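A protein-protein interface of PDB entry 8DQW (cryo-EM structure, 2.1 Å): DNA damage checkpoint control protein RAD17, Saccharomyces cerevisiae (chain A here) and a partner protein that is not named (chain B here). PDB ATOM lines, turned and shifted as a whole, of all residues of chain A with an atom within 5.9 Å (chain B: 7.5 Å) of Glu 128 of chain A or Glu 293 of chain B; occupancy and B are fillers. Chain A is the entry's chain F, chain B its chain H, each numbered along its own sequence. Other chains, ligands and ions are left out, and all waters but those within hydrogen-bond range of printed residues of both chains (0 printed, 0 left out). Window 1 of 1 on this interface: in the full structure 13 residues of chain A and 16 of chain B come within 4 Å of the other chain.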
ATOM      1  N   VAL A  95      -4.743  -4.800   3.207  1.00  0.00           N
ATOM      2  CA  VAL A  95      -3.712  -5.316   4.105  1.00  0.00           C
ATOM      3  C   VAL A  95      -3.297  -6.726   3.694  1.00  0.00           C
ATOM      4  O   VAL A  95      -2.106  -7.059   3.687  1.00  0.00           O
ATOM      5  CB  VAL A  95      -4.194  -5.272   5.565  1.00  0.00           C
ATOM      6  CG1 VAL A  95      -3.121  -5.826   6.486  1.00  0.00           C
ATOM      7  CG2 VAL A  95      -4.550  -3.849   5.965  1.00  0.00           C
ATOM      8  N   MET A  96      -4.266  -7.577   3.346  1.00  0.00           N
ATOM      9  CA  MET A  96      -3.955  -8.964   3.015  1.00  0.00           C
ATOM     10  C   MET A  96      -3.299  -9.094   1.647  1.00  0.00           C
ATOM     11  O   MET A  96      -2.503 -10.014   1.429  1.00  0.00           O
ATOM     12  CB  MET A  96      -5.226  -9.812   3.063  1.00  0.00           C
ATOM     13  CG  MET A  96      -5.909  -9.848   4.422  1.00  0.00           C
ATOM     14  SD  MET A  96      -7.594 -10.488   4.324  1.00  0.00           S
ATOM     15  CE  MET A  96      -7.333 -12.210   4.737  1.00  0.00           C
ATOM     16  N   LEU A 119     -14.047 -14.747   3.954  1.00  0.00           N
ATOM     17  CA  LEU A 119     -13.082 -14.638   2.869  1.00  0.00           C
ATOM     18  C   LEU A 119     -11.745 -15.179   3.355  1.00  0.00           C
ATOM     19  O   LEU A 119     -11.239 -14.744   4.393  1.00  0.00           O
ATOM     20  CB  LEU A 119     -12.948 -13.183   2.404  1.00  0.00           C
ATOM     21  CG  LEU A 119     -11.890 -12.858   1.347  1.00  0.00           C
ATOM     22  CD1 LEU A 119     -12.288 -11.603   0.583  1.00  0.00           C
ATOM     23  CD2 LEU A 119     -10.512 -12.684   1.972  1.00  0.00           C
ATOM     24  N   ILE A 120     -11.174 -16.120   2.606  1.00  0.00           N
ATOM     25  CA  ILE A 120      -9.935 -16.784   2.988  1.00  0.00           C
ATOM     26  C   ILE A 120      -8.928 -16.633   1.860  1.00  0.00           C
ATOM     27  O   ILE A 120      -9.208 -17.008   0.716  1.00  0.00           O
ATOM     28  CB  ILE A 120     -10.161 -18.274   3.311  1.00  0.00           C
ATOM     29  CG1 ILE A 120     -11.043 -18.422   4.550  1.00  0.00           C
ATOM     30  CG2 ILE A 120      -8.830 -18.982   3.523  1.00  0.00           C
ATOM     31  CD1 ILE A 120     -11.699 -19.780   4.675  1.00  0.00           C
ATOM     32  N   PHE A 121      -7.758 -16.089   2.183  1.00  0.00           N
ATOM     33  CA  PHE A 121      -6.625 -16.046   1.269  1.00  0.00           C
ATOM     34  C   PHE A 121      -5.662 -17.160   1.658  1.00  0.00           C
ATOM     35  O   PHE A 121      -5.089 -17.134   2.753  1.00  0.00           O
ATOM     36  CB  PHE A 121      -5.926 -14.686   1.320  1.00  0.00           C
ATOM     37  CG  PHE A 121      -6.561 -13.641   0.445  1.00  0.00           C
ATOM     38  CD1 PHE A 121      -7.908 -13.697   0.128  1.00  0.00           C
ATOM     39  CD2 PHE A 121      -5.804 -12.595  -0.058  1.00  0.00           C
ATOM     40  CE1 PHE A 121      -8.485 -12.734  -0.677  1.00  0.00           C
ATOM     41  CE2 PHE A 121      -6.379 -11.629  -0.861  1.00  0.00           C
ATOM     42  CZ  PHE A 121      -7.720 -11.699  -1.170  1.00  0.00           C
ATOM     43  N   GLU A 122      -5.495 -18.137   0.770  1.00  0.00           N
ATOM     44  CA  GLU A 122      -4.681 -19.319   1.024  1.00  0.00           C
ATOM     45  C   GLU A 122      -3.376 -19.202   0.248  1.00  0.00           C
ATOM     46  O   GLU A 122      -3.387 -19.094  -0.986  1.00  0.00           O
ATOM     47  CB  GLU A 122      -5.428 -20.591   0.625  1.00  0.00           C
ATOM     48  CG  GLU A 122      -5.032 -21.824   1.423  1.00  0.00           C
ATOM     49  CD  GLU A 122      -5.760 -21.931   2.750  1.00  0.00           C
ATOM     50  OE1 GLU A 122      -6.754 -21.202   2.950  1.00  0.00           O
ATOM     51  OE2 GLU A 122      -5.339 -22.749   3.594  1.00  0.00           O
ATOM     52  N   ILE A 126       0.553 -20.397   4.615  1.00  0.00           N
ATOM     53  CA  ILE A 126      -0.165 -19.501   5.514  1.00  0.00           C
ATOM     54  C   ILE A 126      -1.520 -19.185   4.900  1.00  0.00           C
ATOM     55  O   ILE A 126      -1.607 -18.853   3.712  1.00  0.00           O
ATOM     56  CB  ILE A 126       0.626 -18.207   5.779  1.00  0.00           C
ATOM     57  CG1 ILE A 126       1.933 -18.519   6.512  1.00  0.00           C
ATOM     58  CG2 ILE A 126      -0.212 -17.228   6.586  1.00  0.00           C
ATOM     59  CD1 ILE A 126       2.991 -17.450   6.352  1.00  0.00           C
ATOM     60  N   SER A 127      -2.572 -19.286   5.708  1.00  0.00           N
ATOM     61  CA  SER A 127      -3.928 -18.951   5.297  1.00  0.00           C
ATOM     62  C   SER A 127      -4.478 -17.881   6.227  1.00  0.00           C
ATOM     63  O   SER A 127      -4.360 -17.996   7.450  1.00  0.00           O
ATOM     64  CB  SER A 127      -4.835 -20.185   5.318  1.00  0.00           C
ATOM     65  OG  SER A 127      -5.200 -20.526   6.642  1.00  0.00           O
ATOM     66  N   GLU A 128      -5.076 -16.845   5.645  1.00  0.00           N
ATOM     67  CA  GLU A 128      -5.667 -15.746   6.397  1.00  0.00           C
ATOM     68  C   GLU A 128      -7.174 -15.756   6.177  1.00  0.00           C
ATOM     69  O   GLU A 128      -7.639 -15.642   5.038  1.00  0.00           O
ATOM     70  CB  GLU A 128      -5.066 -14.407   5.970  1.00  0.00           C
ATOM     71  CG  GLU A 128      -3.588 -14.264   6.295  1.00  0.00           C
ATOM     72  CD  GLU A 128      -3.167 -12.817   6.463  1.00  0.00           C
ATOM     73  OE1 GLU A 128      -3.619 -11.967   5.669  1.00  0.00           O
ATOM     74  OE2 GLU A 128      -2.386 -12.528   7.392  1.00  0.00           O
ATOM     75  N   ARG A 129      -7.927 -15.884   7.266  1.00  0.00           N
ATOM     76  CA  ARG A 129      -9.380 -15.976   7.230  1.00  0.00           C
ATOM     77  C   ARG A 129      -9.976 -14.742   7.893  1.00  0.00           C
ATOM     78  O   ARG A 129      -9.632 -14.422   9.036  1.00  0.00           O
ATOM     79  CB  ARG A 129      -9.853 -17.247   7.941  1.00  0.00           C
ATOM     80  CG  ARG A 129     -11.365 -17.404   8.074  1.00  0.00           C
ATOM     81  CD  ARG A 129     -11.708 -18.397   9.174  1.00  0.00           C
ATOM     82  NE  ARG A 129     -13.142 -18.484   9.425  1.00  0.00           N
ATOM     83  CZ  ARG A 129     -13.961 -19.352   8.842  1.00  0.00           C
ATOM     84  NH1 ARG A 129     -13.525 -20.223   7.946  1.00  0.00           N
ATOM     85  NH2 ARG A 129     -15.250 -19.345   9.168  1.00  0.00           N
ATOM     86  N   VAL A 130     -10.869 -14.059   7.181  1.00  0.00           N
ATOM     87  CA  VAL A 130     -11.563 -12.885   7.695  1.00  0.00           C
ATOM     88  C   VAL A 130     -13.060 -13.131   7.591  1.00  0.00           C
ATOM     89  O   VAL A 130     -13.536 -13.735   6.624  1.00  0.00           O
ATOM     90  CB  VAL A 130     -11.166 -11.598   6.939  1.00  0.00           C
ATOM     91  CG1 VAL A 130      -9.677 -11.326   7.096  1.00  0.00           C
ATOM     92  CG2 VAL A 130     -11.540 -11.696   5.470  1.00  0.00           C
ATOM     93  N   GLY B 248       7.842 -15.280   8.370  1.00  0.00           N
ATOM     94  CA  GLY B 248       6.798 -14.401   7.870  1.00  0.00           C
ATOM     95  C   GLY B 248       5.485 -14.584   8.607  1.00  0.00           C
ATOM     96  O   GLY B 248       4.757 -13.619   8.850  1.00  0.00           O
ATOM     97  N   PHE B 249       5.164 -15.828   8.971  1.00  0.00           N
ATOM     98  CA  PHE B 249       3.931 -16.097   9.703  1.00  0.00           C
ATOM     99  C   PHE B 249       3.935 -15.413  11.064  1.00  0.00           C
ATOM    100  O   PHE B 249       2.915 -14.862  11.494  1.00  0.00           O
ATOM    101  CB  PHE B 249       3.745 -17.607   9.860  1.00  0.00           C
ATOM    102  CG  PHE B 249       2.762 -17.990  10.927  1.00  0.00           C
ATOM    103  CD1 PHE B 249       1.411 -17.728  10.773  1.00  0.00           C
ATOM    104  CD2 PHE B 249       3.189 -18.622  12.082  1.00  0.00           C
ATOM    105  CE1 PHE B 249       0.506 -18.084  11.754  1.00  0.00           C
ATOM    106  CE2 PHE B 249       2.289 -18.982  13.066  1.00  0.00           C
ATOM    107  CZ  PHE B 249       0.946 -18.712  12.901  1.00  0.00           C
ATOM    108  N   ARG B 252       3.490 -11.597  10.616  1.00  0.00           N
ATOM    109  CA  ARG B 252       2.351 -11.156   9.816  1.00  0.00           C
ATOM    110  C   ARG B 252       1.521 -10.122  10.569  1.00  0.00           C
ATOM    111  O   ARG B 252       1.139  -9.087  10.009  1.00  0.00           O
ATOM    112  CB  ARG B 252       1.493 -12.361   9.432  1.00  0.00           C
ATOM    113  CG  ARG B 252       0.285 -12.030   8.568  1.00  0.00           C
ATOM    114  CD  ARG B 252       0.693 -11.418   7.237  1.00  0.00           C
ATOM    115  NE  ARG B 252       1.620 -12.271   6.504  1.00  0.00           N
ATOM    116  CZ  ARG B 252       1.279 -13.394   5.886  1.00  0.00           C
ATOM    117  NH1 ARG B 252       0.031 -13.831   5.883  1.00  0.00           N
ATOM    118  NH2 ARG B 252       2.216 -14.096   5.253  1.00  0.00           N
ATOM    119  N   VAL B 253       1.251 -10.375  11.852  1.00  0.00           N
ATOM    120  CA  VAL B 253       0.381  -9.496  12.625  1.00  0.00           C
ATOM    121  C   VAL B 253       0.938  -8.083  12.714  1.00  0.00           C
ATOM    122  O   VAL B 253       0.190  -7.143  13.004  1.00  0.00           O
ATOM    123  CB  VAL B 253       0.149 -10.084  14.033  1.00  0.00           C
ATOM    124  CG1 VAL B 253       1.259  -9.661  14.989  1.00  0.00           C
ATOM    125  CG2 VAL B 253      -1.211  -9.658  14.564  1.00  0.00           C
ATOM    126  N   ARG B 255       1.619  -6.234  10.399  1.00  0.00           N
ATOM    127  CA  ARG B 255       1.037  -5.415   9.344  1.00  0.00           C
ATOM    128  C   ARG B 255      -0.139  -4.579   9.838  1.00  0.00           C
ATOM    129  O   ARG B 255      -0.523  -3.618   9.164  1.00  0.00           O
ATOM    130  CB  ARG B 255       0.593  -6.303   8.180  1.00  0.00           C
ATOM    131  CG  ARG B 255       1.750  -6.880   7.376  1.00  0.00           C
ATOM    132  CD  ARG B 255       1.263  -7.730   6.213  1.00  0.00           C
ATOM    133  NE  ARG B 255       2.371  -8.238   5.413  1.00  0.00           N
ATOM    134  CZ  ARG B 255       2.308  -9.307   4.628  1.00  0.00           C
ATOM    135  NH1 ARG B 255       1.194 -10.010   4.503  1.00  0.00           N
ATOM    136  NH2 ARG B 255       3.390  -9.677   3.950  1.00  0.00           N
ATOM    137  N   TYR B 256      -0.710  -4.915  10.993  1.00  0.00           N
ATOM    138  CA  TYR B 256      -1.834  -4.183  11.576  1.00  0.00           C
ATOM    139  C   TYR B 256      -1.300  -3.337  12.728  1.00  0.00           C
ATOM    140  O   TYR B 256      -1.019  -3.853  13.814  1.00  0.00           O
ATOM    141  CB  TYR B 256      -2.923  -5.144  12.042  1.00  0.00           C
ATOM    142  CG  TYR B 256      -3.349  -6.140  10.986  1.00  0.00           C
ATOM    143  CD1 TYR B 256      -2.664  -7.335  10.814  1.00  0.00           C
ATOM    144  CD2 TYR B 256      -4.435  -5.884  10.161  1.00  0.00           C
ATOM    145  CE1 TYR B 256      -3.049  -8.247   9.851  1.00  0.00           C
ATOM    146  CE2 TYR B 256      -4.830  -6.790   9.197  1.00  0.00           C
ATOM    147  CZ  TYR B 256      -4.133  -7.969   9.044  1.00  0.00           C
ATOM    148  OH  TYR B 256      -4.521  -8.874   8.084  1.00  0.00           O
ATOM    149  N   MET B 265      -3.421 -19.723  19.727  1.00  0.00           N
ATOM    150  CA  MET B 265      -4.186 -20.944  19.939  1.00  0.00           C
ATOM    151  C   MET B 265      -3.430 -22.122  19.343  1.00  0.00           C
ATOM    152  O   MET B 265      -2.828 -22.005  18.273  1.00  0.00           O
ATOM    153  CB  MET B 265      -5.581 -20.836  19.308  1.00  0.00           C
ATOM    154  CG  MET B 265      -6.396 -22.122  19.342  1.00  0.00           C
ATOM    155  SD  MET B 265      -7.980 -21.956  18.497  1.00  0.00           S
ATOM    156  CE  MET B 265      -8.947 -21.112  19.743  1.00  0.00           C
ATOM    157  N   LYS B 282      -2.498 -21.094  15.561  1.00  0.00           N
ATOM    158  CA  LYS B 282      -3.238 -19.988  14.972  1.00  0.00           C
ATOM    159  C   LYS B 282      -3.045 -18.724  15.799  1.00  0.00           C
ATOM    160  O   LYS B 282      -2.885 -18.775  17.023  1.00  0.00           O
ATOM    161  CB  LYS B 282      -4.742 -20.294  14.872  1.00  0.00           C
ATOM    162  CG  LYS B 282      -5.090 -21.771  14.762  1.00  0.00           C
ATOM    163  CD  LYS B 282      -6.363 -21.989  13.951  1.00  0.00           C
ATOM    164  CE  LYS B 282      -7.587 -21.384  14.626  1.00  0.00           C
ATOM    165  NZ  LYS B 282      -8.175 -22.299  15.641  1.00  0.00           N
ATOM    166  N   ILE B 283      -3.073 -17.586  15.110  1.00  0.00           N
ATOM    167  CA  ILE B 283      -3.030 -16.265  15.728  1.00  0.00           C
ATOM    168  C   ILE B 283      -4.337 -15.562  15.386  1.00  0.00           C
ATOM    169  O   ILE B 283      -4.648 -15.362  14.207  1.00  0.00           O
ATOM    170  CB  ILE B 283      -1.824 -15.445  15.245  1.00  0.00           C
ATOM    171  CG1 ILE B 283      -0.517 -16.175  15.568  1.00  0.00           C
ATOM    172  CG2 ILE B 283      -1.836 -14.054  15.874  1.00  0.00           C
ATOM    173  CD1 ILE B 283       0.708 -15.543  14.947  1.00  0.00           C
ATOM    174  N   ILE B 284      -5.091 -15.177  16.411  1.00  0.00           N
ATOM    175  CA  ILE B 284      -6.407 -14.574  16.245  1.00  0.00           C
ATOM    176  C   ILE B 284      -6.329 -13.115  16.670  1.00  0.00           C
ATOM    177  O   ILE B 284      -5.736 -12.789  17.709  1.00  0.00           O
ATOM    178  CB  ILE B 284      -7.479 -15.334  17.046  1.00  0.00           C
ATOM    179  CG1 ILE B 284      -7.601 -16.774  16.537  1.00  0.00           C
ATOM    180  CG2 ILE B 284      -8.820 -14.623  16.953  1.00  0.00           C
ATOM    181  CD1 ILE B 284      -8.281 -17.711  17.512  1.00  0.00           C
ATOM    182  N   VAL B 285      -6.905 -12.241  15.846  1.00  0.00           N
ATOM    183  CA  VAL B 285      -7.013 -10.814  16.122  1.00  0.00           C
ATOM    184  C   VAL B 285      -8.491 -10.454  16.078  1.00  0.00           C
ATOM    185  O   VAL B 285      -9.166 -10.690  15.064  1.00  0.00           O
ATOM    186  CB  VAL B 285      -6.213  -9.975  15.112  1.00  0.00           C
ATOM    187  CG1 VAL B 285      -6.466  -8.487  15.332  1.00  0.00           C
ATOM    188  CG2 VAL B 285      -4.730 -10.294  15.212  1.00  0.00           C
ATOM    189  N   ASN B 286      -8.992  -9.887  17.177  1.00  0.00           N
ATOM    190  CA  ASN B 286     -10.384  -9.467  17.291  1.00  0.00           C
ATOM    191  C   ASN B 286     -10.503  -7.999  17.683  1.00  0.00           C
ATOM    192  O   ASN B 286     -11.558  -7.572  18.164  1.00  0.00           O
ATOM    193  CB  ASN B 286     -11.122 -10.347  18.300  1.00  0.00           C
ATOM    194  CG  ASN B 286     -10.387 -10.461  19.617  1.00  0.00           C
ATOM    195  OD1 ASN B 286     -10.419  -9.546  20.440  1.00  0.00           O
ATOM    196  ND2 ASN B 286      -9.715 -11.587  19.823  1.00  0.00           N
ATOM    197  N   TRP B 290     -13.270  -6.357  11.730  1.00  0.00           N
ATOM    198  CA  TRP B 290     -13.564  -7.684  11.212  1.00  0.00           C
ATOM    199  C   TRP B 290     -12.681  -8.698  11.922  1.00  0.00           C
ATOM    200  O   TRP B 290     -11.518  -8.414  12.223  1.00  0.00           O
ATOM    201  CB  TRP B 290     -13.324  -7.748   9.701  1.00  0.00           C
ATOM    202  CG  TRP B 290     -11.927  -7.365   9.326  1.00  0.00           C
ATOM    203  CD1 TRP B 290     -10.857  -8.201   9.189  1.00  0.00           C
ATOM    204  CD2 TRP B 290     -11.442  -6.045   9.056  1.00  0.00           C
ATOM    205  NE1 TRP B 290      -9.737  -7.483   8.845  1.00  0.00           N
ATOM    206  CE2 TRP B 290     -10.070  -6.158   8.759  1.00  0.00           C
ATOM    207  CE3 TRP B 290     -12.036  -4.779   9.035  1.00  0.00           C
ATOM    208  CZ2 TRP B 290      -9.283  -5.054   8.439  1.00  0.00           C
ATOM    209  CZ3 TRP B 290     -11.252  -3.685   8.718  1.00  0.00           C
ATOM    210  CH2 TRP B 290      -9.890  -3.829   8.427  1.00  0.00           C
ATOM    211  N   HIS B 291     -13.235  -9.877  12.193  1.00  0.00           N
ATOM    212  CA  HIS B 291     -12.463 -10.934  12.834  1.00  0.00           C
ATOM    213  C   HIS B 291     -11.366 -11.425  11.899  1.00  0.00           C
ATOM    214  O   HIS B 291     -11.586 -11.598  10.697  1.00  0.00           O
ATOM    215  CB  HIS B 291     -13.380 -12.090  13.229  1.00  0.00           C
ATOM    216  CG  HIS B 291     -12.715 -13.125  14.084  1.00  0.00           C
ATOM    217  ND1 HIS B 291     -12.553 -12.976  15.444  1.00  0.00           N
ATOM    218  CD2 HIS B 291     -12.176 -14.327  13.771  1.00  0.00           C
ATOM    219  CE1 HIS B 291     -11.941 -14.041  15.932  1.00  0.00           C
ATOM    220  NE2 HIS B 291     -11.701 -14.876  14.937  1.00  0.00           N
ATOM    221  N   LEU B 292     -10.172 -11.649  12.453  1.00  0.00           N
ATOM    222  CA  LEU B 292      -9.025 -12.077  11.661  1.00  0.00           C
ATOM    223  C   LEU B 292      -8.392 -13.309  12.289  1.00  0.00           C
ATOM    224  O   LEU B 292      -8.177 -13.351  13.504  1.00  0.00           O
ATOM    225  CB  LEU B 292      -7.990 -10.952  11.539  1.00  0.00           C
ATOM    226  CG  LEU B 292      -6.646 -11.320  10.904  1.00  0.00           C
ATOM    227  CD1 LEU B 292      -6.829 -11.863   9.492  1.00  0.00           C
ATOM    228  CD2 LEU B 292      -5.722 -10.115  10.897  1.00  0.00           C
ATOM    229  N   GLU B 293      -8.091 -14.305  11.458  1.00  0.00           N
ATOM    230  CA  GLU B 293      -7.384 -15.506  11.882  1.00  0.00           C
ATOM    231  C   GLU B 293      -6.247 -15.774  10.907  1.00  0.00           C
ATOM    232  O   GLU B 293      -6.445 -15.718   9.690  1.00  0.00           O
ATOM    233  CB  GLU B 293      -8.323 -16.715  11.941  1.00  0.00           C
ATOM    234  CG  GLU B 293      -9.429 -16.595  12.976  1.00  0.00           C
ATOM    235  CD  GLU B 293     -10.017 -17.939  13.362  1.00  0.00           C
ATOM    236  OE1 GLU B 293     -10.173 -18.801  12.470  1.00  0.00           O
ATOM    237  OE2 GLU B 293     -10.324 -18.135  14.556  1.00  0.00           O
ATOM    238  N   ILE B 294      -5.062 -16.059  11.441  1.00  0.00           N
ATOM    239  CA  ILE B 294      -3.890 -16.407  10.646  1.00  0.00           C
ATOM    240  C   ILE B 294      -3.451 -17.798  11.079  1.00  0.00           C
ATOM    241  O   ILE B 294      -3.097 -18.006  12.246  1.00  0.00           O
ATOM    242  CB  ILE B 294      -2.751 -15.391  10.821  1.00  0.00           C
ATOM    243  CG1 ILE B 294      -3.254 -13.962  10.590  1.00  0.00           C
ATOM    244  CG2 ILE B 294      -1.613 -15.702   9.861  1.00  0.00           C
ATOM    245  CD1 ILE B 294      -2.360 -12.899  11.185  1.00  0.00           C
ATOM    246  N   CYS B 295      -3.468 -18.742  10.145  1.00  0.00           N
ATOM    247  CA  CYS B 295      -3.223 -20.146  10.440  1.00  0.00           C
ATOM    248  C   CYS B 295      -1.946 -20.609   9.755  1.00  0.00           C
ATOM    249  O   CYS B 295      -1.653 -20.206   8.625  1.00  0.00           O
ATOM    250  CB  CYS B 295      -4.400 -21.015   9.983  1.00  0.00           C
ATOM    251  SG  CYS B 295      -4.574 -22.569  10.890  1.00  0.00           S
ATOM    252  N   ASN B 297      -0.239 -23.764   8.144  1.00  0.00           N
ATOM    253  CA  ASN B 297      -0.589 -25.054   7.567  1.00  0.00           C
ATOM    254  C   ASN B 297       0.627 -25.926   7.286  1.00  0.00           C
ATOM    255  O   ASN B 297       0.465 -27.060   6.826  1.00  0.00           O
ATOM    256  CB  ASN B 297      -1.383 -24.846   6.274  1.00  0.00           C
ATOM    257  CG  ASN B 297      -2.435 -23.764   6.408  1.00  0.00           C
ATOM    258  OD1 ASN B 297      -3.383 -23.895   7.181  1.00  0.00           O
ATOM    259  ND2 ASN B 297      -2.270 -22.684   5.655  1.00  0.00           N
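O of Ser 127 of chain A is in hydrogen-bond range of N of Cys 295 of chain B (2.9 Å). N of Ser 127 of chain A lies close to ND2 of Asn 297 of chain B (3.4 Å). OE2 of Glu 128 of chain A lies within salt-bridge range of NH1 of Arg 252 of chain B, 3.1 Å away. The backbone carbonyl oxygen (O) of Glu 293 of chain B sits at hydrogen-bond distance from the backbone NH (N) of Arg 129 of chain A (2.8 Å).
N of Val 130 of chain A is in hydrogen-bond range of O of Leu 119 of chain A, 2.9 Å away. N of Phe 121 of chain A sits at hydrogen-bond distance from O of Glu 128 of chain A, at 2.9 Å. The backbone NH (N) of Ile 294 of chain B lies within hydrogen-bond range of the backbone carbonyl oxygen (O) of Ile 283 of chain B. O of Leu 292 of chain B is in hydrogen-bond range of N of Val 285 of chain B, at 2.9 Å.
Among the printed residues, pairs that only touch across the chains: Val 95 of chain A with Tyr 256 of chain B (3.3 Å), Glu 122 of chain A with Asn 297 of chain B (3.7 Å), Ile 126 of chain A with Phe 249 of chain B (3.6 Å), Ile 126 of chain A with Arg 252 of chain B (3.5 Å), Ile 126 of chain A with Ile 294 of chain B (3.9 Å), Ile 126 of chain A with Cys 295 of chain B (3.5 Å), Ile 126 of chain A with Asn 297 of chain B (3.7 Å), Ser 127 of chain A with Glu 293 of chain B (3.8 Å), Ser 127 of chain A with Ile 294 of chain B (3.6 Å), Glu 128 of chain A with Glu 293 of chain B (3.4 Å), Glu 128 of chain A with Ile 294 of chain B (3.6 Å), Arg 129 of chain A with His 291 of chain B (3.8 Å), Arg 129 of chain A with Leu 292 of chain B (3.6 Å), Val 130 of chain A with Trp 290 of chain B (3.9 Å), Val 130 of chain A with His 291 of chain B (3.3 Å) and Val 130 of chain A with Leu 292 of chain B (3.8 Å).
Of chain A, only Ser 127 (3.8 Å), Glu 128 (3.4 Å) and Arg 129 (2.8 Å) come within 4 Å of Glu 293 of chain B. Of the printed residues of chain B, Ser 127 of chain A touches Glu 293, Ile 294, Cys 295 and Asn 297. Of the printed residues of chain A, Trp 290 of chain B touches Val 130. Lys 282 of chain B touches none of the printed residues of chain A. Leu 119 of chain A touches none of the printed residues of chain B. The nearest residue of chain B that does not touch Glu 128 of chain A is Tyr 256 of chain B (4.03 Å). The nearest residue of chain A that does not touch Glu 293 of chain B is Val 130 of chain A (5.1 Å).
Hydrophobic or aromatic side chains of chain B within 4 Å of the printed part of chain A: Phe 249, Tyr 256, Trp 290, Leu 292 and Ile 294. Of the 11 printed residues of chain A, 7 touch a printed residue of chain B. Hydrophobic or aromatic side chains of chain A within 4 Å of the printed part of chain B: Val 95, Ile 126 and Val 130. Along chain A the printed residues that touch a printed residue of chain B span positions 95 to 130. Among the printed residues, 20 pairs touch across the chains. Among the printed residues, Asp or Glu carboxylates within 4 Å of a Lys or Arg side-chain nitrogen of the other chain: Glu 128 of chain A with Arg 252 of chain B (3.1 Å).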
